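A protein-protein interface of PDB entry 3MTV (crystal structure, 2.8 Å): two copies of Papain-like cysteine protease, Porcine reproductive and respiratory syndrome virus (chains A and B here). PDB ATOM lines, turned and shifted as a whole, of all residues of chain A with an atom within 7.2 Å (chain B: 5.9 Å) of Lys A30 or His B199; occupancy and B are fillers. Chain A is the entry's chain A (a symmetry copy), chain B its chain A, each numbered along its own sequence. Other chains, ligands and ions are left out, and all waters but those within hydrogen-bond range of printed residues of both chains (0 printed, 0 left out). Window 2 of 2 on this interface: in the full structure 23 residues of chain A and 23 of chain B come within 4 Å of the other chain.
No position is printed for both chains. Of the 9 pairs that touch across the chains among the printed residues, none has its exchanged pair printed and touching as well.
The backbone carbonyl oxygen (O) of Lys B200 lies close to the backbone carbonyl oxygen (O) of Pro B122 (2.4 Å). The backbone carbonyl oxygen (O) of Glu B154 lies within hydrogen-bond range of the side-chain amino group (NZ) of Lys B200 (3.5 Å). The backbone carbonyl oxygen (O) of Ser B155 is in hydrogen-bond range of the side-chain amino group (NZ) of Lys B200, at 3.0 Å. N of Trp B201 is in hydrogen-bond range of O of Trp B156, 3.0 Å away. The backbone NH (N) of Asp A5 lies within hydrogen-bond range of the backbone carbonyl oxygen (O) of Glu A32 (2.9 Å). O of Val A29 sits close to NE of Arg A24, at 3.4 Å.
Lys A30 touches just these residues of chain B: Trp B156 (3.4 Å) and His B199 (3.7 Å). Of chain A, only Lys A30 comes within 4 Å of His B199. Of the printed residues of chain A, Lys B200 touches Glu A32. Of the printed residues of chain A, Trp B156 touches Glu A28, Val A29, Lys A30 and Phe A31.
Trp B156 touches Glu A28. Val A29 touches Trp B156. Lys A30 touches Trp B156 (O to CE3, 3.4 Å). Lys A30 touches His B199. Phe A31 touches Glu B154. Phe A31 touches Ser B155 (CD2 to CA, 3.98 Å). Phe A31 touches Trp B156 (CZ to CZ3, 3.7 Å). Glu A32 touches Glu B154. NZ of Lys B200 touches CG of Glu A32, 3.9 Å away.
Of the 10 printed residues of chain B, 5 touch a printed residue of chain A. Hydrophobic or aromatic side chains of chain B that line the printed part of chain A: Trp B156 and His B199. Along chain B the printed residues that touch a printed residue of chain A span positions 154 to 200. Along chain A the printed residues that touch a printed residue of chain B span positions 28 to 32.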
ATOM      1  N   ASP A   5      11.097 -11.204  -5.374  1.00  0.00           N
ATOM      2  CA  ASP A   5      10.565 -12.537  -5.279  1.00  0.00           C
ATOM      3  C   ASP A   5      11.726 -13.528  -5.260  1.00  0.00           C
ATOM      4  O   ASP A   5      12.626 -13.428  -6.091  1.00  0.00           O
ATOM      5  CB  ASP A   5       9.737 -12.810  -6.525  1.00  0.00           C
ATOM      6  CG  ASP A   5       9.037 -14.173  -6.497  1.00  0.00           C
ATOM      7  OD1 ASP A   5       7.741 -14.278  -6.597  1.00  0.00           O
ATOM      8  OD2 ASP A   5       9.826 -15.144  -6.412  1.00  0.00           O
ATOM      9  N   VAL A  11       9.267 -13.522  -0.235  1.00  0.00           N
ATOM     10  CA  VAL A  11       9.919 -12.432  -0.899  1.00  0.00           C
ATOM     11  C   VAL A  11      10.875 -11.813   0.061  1.00  0.00           C
ATOM     12  O   VAL A  11      10.778 -12.083   1.217  1.00  0.00           O
ATOM     13  CB  VAL A  11       8.910 -11.305  -1.213  1.00  0.00           C
ATOM     14  CG1 VAL A  11       7.977 -11.717  -2.272  1.00  0.00           C
ATOM     15  CG2 VAL A  11       8.141 -10.852   0.029  1.00  0.00           C
ATOM     16  N   ARG A  24       4.495 -14.380   0.220  1.00  0.00           N
ATOM     17  CA  ARG A  24       4.480 -13.697  -1.072  1.00  0.00           C
ATOM     18  C   ARG A  24       3.176 -12.994  -0.908  1.00  0.00           C
ATOM     19  O   ARG A  24       3.097 -11.724  -0.864  1.00  0.00           O
ATOM     20  CB  ARG A  24       4.479 -14.701  -2.255  1.00  0.00           C
ATOM     21  CG  ARG A  24       4.193 -14.210  -3.717  1.00  0.00           C
ATOM     22  CD  ARG A  24       4.403 -15.442  -4.724  1.00  0.00           C
ATOM     23  NE  ARG A  24       3.599 -15.387  -5.984  1.00  0.00           N
ATOM     24  CZ  ARG A  24       4.039 -15.267  -7.286  1.00  0.00           C
ATOM     25  NH1 ARG A  24       5.388 -15.188  -7.664  1.00  0.00           N
ATOM     26  NH2 ARG A  24       3.074 -15.238  -8.262  1.00  0.00           N
ATOM     27  N   GLY A  26      -0.810 -13.625  -2.664  1.00  0.00           N
ATOM     28  CA  GLY A  26      -1.419 -14.216  -3.851  1.00  0.00           C
ATOM     29  C   GLY A  26      -0.683 -14.018  -5.198  1.00  0.00           C
ATOM     30  O   GLY A  26       0.445 -13.328  -5.345  1.00  0.00           O
ATOM     31  N   ASN A  27      -1.331 -14.610  -6.210  1.00  0.00           N
ATOM     32  CA  ASN A  27      -0.642 -14.713  -7.505  1.00  0.00           C
ATOM     33  C   ASN A  27      -0.421 -13.369  -8.093  1.00  0.00           C
ATOM     34  O   ASN A  27       0.165 -13.274  -9.149  1.00  0.00           O
ATOM     35  CB  ASN A  27      -1.423 -15.478  -8.561  1.00  0.00           C
ATOM     36  CG  ASN A  27      -1.887 -16.793  -8.070  1.00  0.00           C
ATOM     37  OD1 ASN A  27      -1.059 -17.645  -7.652  1.00  0.00           O
ATOM     38  ND2 ASN A  27      -3.232 -16.991  -8.084  1.00  0.00           N
ATOM     39  N   GLU A  28      -0.981 -12.344  -7.477  1.00  0.00           N
ATOM     40  CA  GLU A  28      -0.847 -11.005  -7.995  1.00  0.00           C
ATOM     41  C   GLU A  28       0.452 -10.459  -7.444  1.00  0.00           C
ATOM     42  O   GLU A  28       1.033  -9.504  -7.977  1.00  0.00           O
ATOM     43  CB  GLU A  28      -1.989 -10.101  -7.551  1.00  0.00           C
ATOM     44  CG  GLU A  28      -1.691  -9.433  -6.144  1.00  0.00           C
ATOM     45  CD  GLU A  28      -2.578  -9.907  -4.916  1.00  0.00           C
ATOM     46  OE1 GLU A  28      -3.346 -10.934  -4.953  1.00  0.00           O
ATOM     47  OE2 GLU A  28      -2.508  -9.203  -3.872  1.00  0.00           O
ATOM     48  N   VAL A  29       0.931 -11.041  -6.357  1.00  0.00           N
ATOM     49  CA  VAL A  29       2.168 -10.482  -5.905  1.00  0.00           C
ATOM     50  C   VAL A  29       3.321 -10.958  -6.762  1.00  0.00           C
ATOM     51  O   VAL A  29       3.568 -12.146  -6.856  1.00  0.00           O
ATOM     52  CB  VAL A  29       2.472 -10.835  -4.541  1.00  0.00           C
ATOM     53  CG1 VAL A  29       3.717 -10.137  -4.285  1.00  0.00           C
ATOM     54  CG2 VAL A  29       1.409 -10.325  -3.599  1.00  0.00           C
ATOM     55  N   LYS A  30       3.986 -10.038  -7.426  1.00  0.00           N
ATOM     56  CA  LYS A  30       4.912 -10.393  -8.514  1.00  0.00           C
ATOM     57  C   LYS A  30       5.948  -9.362  -8.698  1.00  0.00           C
ATOM     58  O   LYS A  30       5.790  -8.449  -9.435  1.00  0.00           O
ATOM     59  CB  LYS A  30       4.222 -10.661  -9.859  1.00  0.00           C
ATOM     60  CG  LYS A  30       3.226 -11.856  -9.775  1.00  0.00           C
ATOM     61  CD  LYS A  30       2.954 -12.383 -11.160  1.00  0.00           C
ATOM     62  CE  LYS A  30       2.603 -13.891 -11.238  1.00  0.00           C
ATOM     63  NZ  LYS A  30       1.529 -14.124 -12.303  1.00  0.00           N
ATOM     64  N   PHE A  31       7.042  -9.520  -7.997  1.00  0.00           N
ATOM     65  CA  PHE A  31       8.106  -8.581  -8.129  1.00  0.00           C
ATOM     66  C   PHE A  31       9.211  -9.178  -8.948  1.00  0.00           C
ATOM     67  O   PHE A  31       9.211 -10.366  -9.247  1.00  0.00           O
ATOM     68  CB  PHE A  31       8.789  -8.396  -6.759  1.00  0.00           C
ATOM     69  CG  PHE A  31       7.968  -7.714  -5.747  1.00  0.00           C
ATOM     70  CD1 PHE A  31       7.149  -8.408  -4.908  1.00  0.00           C
ATOM     71  CD2 PHE A  31       8.012  -6.342  -5.610  1.00  0.00           C
ATOM     72  CE1 PHE A  31       6.346  -7.684  -3.938  1.00  0.00           C
ATOM     73  CE2 PHE A  31       7.208  -5.679  -4.695  1.00  0.00           C
ATOM     74  CZ  PHE A  31       6.393  -6.358  -3.870  1.00  0.00           C
ATOM     75  N   GLU A  32      10.244  -8.353  -9.118  1.00  0.00           N
ATOM     76  CA  GLU A  32      11.502  -8.721  -9.725  1.00  0.00           C
ATOM     77  C   GLU A  32      12.218  -9.857  -9.025  1.00  0.00           C
ATOM     78  O   GLU A  32      12.140  -9.951  -7.815  1.00  0.00           O
ATOM     79  CB  GLU A  32      12.373  -7.485  -9.805  1.00  0.00           C
ATOM     80  CG  GLU A  32      11.968  -6.594 -10.979  1.00  0.00           C
ATOM     81  CD  GLU A  32      12.878  -5.350 -11.093  1.00  0.00           C
ATOM     82  OE1 GLU A  32      14.077  -5.493 -10.502  1.00  0.00           O
ATOM     83  OE2 GLU A  32      12.357  -4.300 -11.750  1.00  0.00           O
ATOM     84  N   PRO A  33      12.901 -10.736  -9.774  1.00  0.00           N
ATOM     85  CA  PRO A  33      13.495 -11.701  -8.898  1.00  0.00           C
ATOM     86  C   PRO A  33      14.824 -11.255  -8.486  1.00  0.00           C
ATOM     87  O   PRO A  33      15.284 -10.176  -8.841  1.00  0.00           O
ATOM     88  CB  PRO A  33      13.602 -12.939  -9.753  1.00  0.00           C
ATOM     89  CG  PRO A  33      12.620 -12.786 -10.747  1.00  0.00           C
ATOM     90  CD  PRO A  33      12.634 -11.340 -11.066  1.00  0.00           C
ATOM     91  N   PRO B 122      -1.181  -5.133 -19.128  1.00  0.00           N
ATOM     92  CA  PRO B 122       0.071  -5.781 -18.791  1.00  0.00           C
ATOM     93  C   PRO B 122       1.376  -5.210 -19.273  1.00  0.00           C
ATOM     94  O   PRO B 122       2.246  -4.990 -18.446  1.00  0.00           O
ATOM     95  CB  PRO B 122      -0.126  -7.188 -19.283  1.00  0.00           C
ATOM     96  CG  PRO B 122      -1.573  -7.410 -19.240  1.00  0.00           C
ATOM     97  CD  PRO B 122      -2.184  -6.105 -19.571  1.00  0.00           C
ATOM     98  N   LYS B 124       3.491  -6.628 -21.728  1.00  0.00           N
ATOM     99  CA  LYS B 124       3.592  -7.411 -22.936  1.00  0.00           C
ATOM    100  C   LYS B 124       2.472  -6.943 -23.885  1.00  0.00           C
ATOM    101  O   LYS B 124       2.620  -6.959 -25.092  1.00  0.00           O
ATOM    102  CB  LYS B 124       3.482  -8.881 -22.655  1.00  0.00           C
ATOM    103  CG  LYS B 124       4.827  -9.567 -22.243  1.00  0.00           C
ATOM    104  CD  LYS B 124       4.567 -10.944 -21.402  1.00  0.00           C
ATOM    105  CE  LYS B 124       3.989 -10.667 -19.882  1.00  0.00           C
ATOM    106  NZ  LYS B 124       3.828 -11.897 -18.970  1.00  0.00           N
ATOM    107  N   GLU B 154      10.769  -2.271  -7.552  1.00  0.00           N
ATOM    108  CA  GLU B 154      10.612  -3.560  -8.221  1.00  0.00           C
ATOM    109  C   GLU B 154       9.211  -3.953  -8.263  1.00  0.00           C
ATOM    110  O   GLU B 154       8.928  -5.060  -8.599  1.00  0.00           O
ATOM    111  CB  GLU B 154      11.565  -4.727  -7.788  1.00  0.00           C
ATOM    112  CG  GLU B 154      12.223  -4.647  -6.429  1.00  0.00           C
ATOM    113  CD  GLU B 154      13.296  -3.631  -6.301  1.00  0.00           C
ATOM    114  OE1 GLU B 154      13.139  -2.729  -5.520  1.00  0.00           O
ATOM    115  OE2 GLU B 154      14.324  -3.720  -6.953  1.00  0.00           O
ATOM    116  N   SER B 155       8.322  -3.026  -7.921  1.00  0.00           N
ATOM    117  CA  SER B 155       6.882  -3.344  -7.964  1.00  0.00           C
ATOM    118  C   SER B 155       6.460  -3.658  -9.373  1.00  0.00           C
ATOM    119  O   SER B 155       7.038  -3.162 -10.389  1.00  0.00           O
ATOM    120  CB  SER B 155       6.057  -2.161  -7.494  1.00  0.00           C
ATOM    121  OG  SER B 155       4.659  -2.374  -7.578  1.00  0.00           O
ATOM    122  N   TRP B 156       5.398  -4.432  -9.395  1.00  0.00           N
ATOM    123  CA  TRP B 156       4.610  -4.533 -10.601  1.00  0.00           C
ATOM    124  C   TRP B 156       3.590  -3.438 -10.919  1.00  0.00           C
ATOM    125  O   TRP B 156       2.811  -3.611 -11.862  1.00  0.00           O
ATOM    126  CB  TRP B 156       3.797  -5.814 -10.636  1.00  0.00           C
ATOM    127  CG  TRP B 156       2.702  -5.847  -9.737  1.00  0.00           C
ATOM    128  CD1 TRP B 156       1.366  -5.623 -10.009  1.00  0.00           C
ATOM    129  CD2 TRP B 156       2.773  -6.146  -8.364  1.00  0.00           C
ATOM    130  NE1 TRP B 156       0.606  -5.772  -8.868  1.00  0.00           N
ATOM    131  CE2 TRP B 156       1.453  -6.078  -7.841  1.00  0.00           C
ATOM    132  CE3 TRP B 156       3.826  -6.457  -7.503  1.00  0.00           C
ATOM    133  CZ2 TRP B 156       1.181  -6.338  -6.527  1.00  0.00           C
ATOM    134  CZ3 TRP B 156       3.530  -6.701  -6.175  1.00  0.00           C
ATOM    135  CH2 TRP B 156       2.234  -6.646  -5.704  1.00  0.00           C
ATOM    136  N   GLY B 197       8.771  -4.550 -19.544  1.00  0.00           N
ATOM    137  CA  GLY B 197       8.881  -5.628 -18.580  1.00  0.00           C
ATOM    138  C   GLY B 197       7.777  -6.684 -18.672  1.00  0.00           C
ATOM    139  O   GLY B 197       6.656  -6.408 -19.192  1.00  0.00           O
ATOM    140  N   SER B 198       8.042  -7.883 -18.120  1.00  0.00           N
ATOM    141  CA  SER B 198       6.936  -8.880 -18.090  1.00  0.00           C
ATOM    142  C   SER B 198       6.393  -8.763 -16.704  1.00  0.00           C
ATOM    143  O   SER B 198       7.169  -8.398 -15.729  1.00  0.00           O
ATOM    144  CB  SER B 198       7.399 -10.322 -18.341  1.00  0.00           C
ATOM    145  OG  SER B 198       7.325 -10.675 -19.712  1.00  0.00           O
ATOM    146  N   HIS B 199       5.091  -8.974 -16.579  1.00  0.00           N
ATOM    147  CA  HIS B 199       4.608  -8.867 -15.217  1.00  0.00           C
ATOM    148  C   HIS B 199       4.584  -7.431 -14.632  1.00  0.00           C
ATOM    149  O   HIS B 199       4.352  -7.251 -13.492  1.00  0.00           O
ATOM    150  CB  HIS B 199       5.544  -9.731 -14.352  1.00  0.00           C
ATOM    151  CG  HIS B 199       5.395 -11.191 -14.610  1.00  0.00           C
ATOM    152  ND1 HIS B 199       6.453 -11.995 -14.947  1.00  0.00           N
ATOM    153  CD2 HIS B 199       4.291 -11.984 -14.624  1.00  0.00           C
ATOM    154  CE1 HIS B 199       6.008 -13.228 -15.150  1.00  0.00           C
ATOM    155  NE2 HIS B 199       4.701 -13.248 -14.959  1.00  0.00           N
ATOM    156  N   LYS B 200       4.906  -6.424 -15.399  1.00  0.00           N
ATOM    157  CA  LYS B 200       4.663  -5.078 -15.016  1.00  0.00           C
ATOM    158  C   LYS B 200       3.210  -4.789 -15.418  1.00  0.00           C
ATOM    159  O   LYS B 200       2.584  -5.604 -16.110  1.00  0.00           O
ATOM    160  CB  LYS B 200       5.606  -4.290 -15.836  1.00  0.00           C
ATOM    161  CG  LYS B 200       6.881  -3.927 -15.121  1.00  0.00           C
ATOM    162  CD  LYS B 200       7.195  -4.923 -14.186  1.00  0.00           C
ATOM    163  CE  LYS B 200       8.131  -4.295 -13.177  1.00  0.00           C
ATOM    164  NZ  LYS B 200       8.449  -5.286 -12.056  1.00  0.00           N
ATOM    165  N   TRP B 201       2.635  -3.706 -14.903  1.00  0.00           N
ATOM    166  CA  TRP B 201       1.303  -3.205 -15.317  1.00  0.00           C
ATOM    167  C   TRP B 201       1.273  -1.729 -15.354  1.00  0.00           C
ATOM    168  O   TRP B 201       2.014  -1.091 -14.606  1.00  0.00           O
ATOM    169  CB  TRP B 201       0.171  -3.592 -14.432  1.00  0.00           C
ATOM    170  CG  TRP B 201      -0.075  -5.056 -14.492  1.00  0.00           C
ATOM    171  CD1 TRP B 201       0.788  -6.101 -14.072  1.00  0.00           C
ATOM    172  CD2 TRP B 201      -1.262  -5.699 -14.948  1.00  0.00           C
ATOM    173  NE1 TRP B 201       0.168  -7.356 -14.247  1.00  0.00           N
ATOM    174  CE2 TRP B 201      -1.072  -7.123 -14.815  1.00  0.00           C
ATOM    175  CE3 TRP B 201      -2.477  -5.222 -15.470  1.00  0.00           C
ATOM    176  CZ2 TRP B 201      -2.013  -8.037 -15.218  1.00  0.00           C
ATOM    177  CZ3 TRP B 201      -3.459  -6.145 -15.855  1.00  0.00           C
ATOM    178  CH2 TRP B 201      -3.202  -7.568 -15.738  1.00  0.00           C
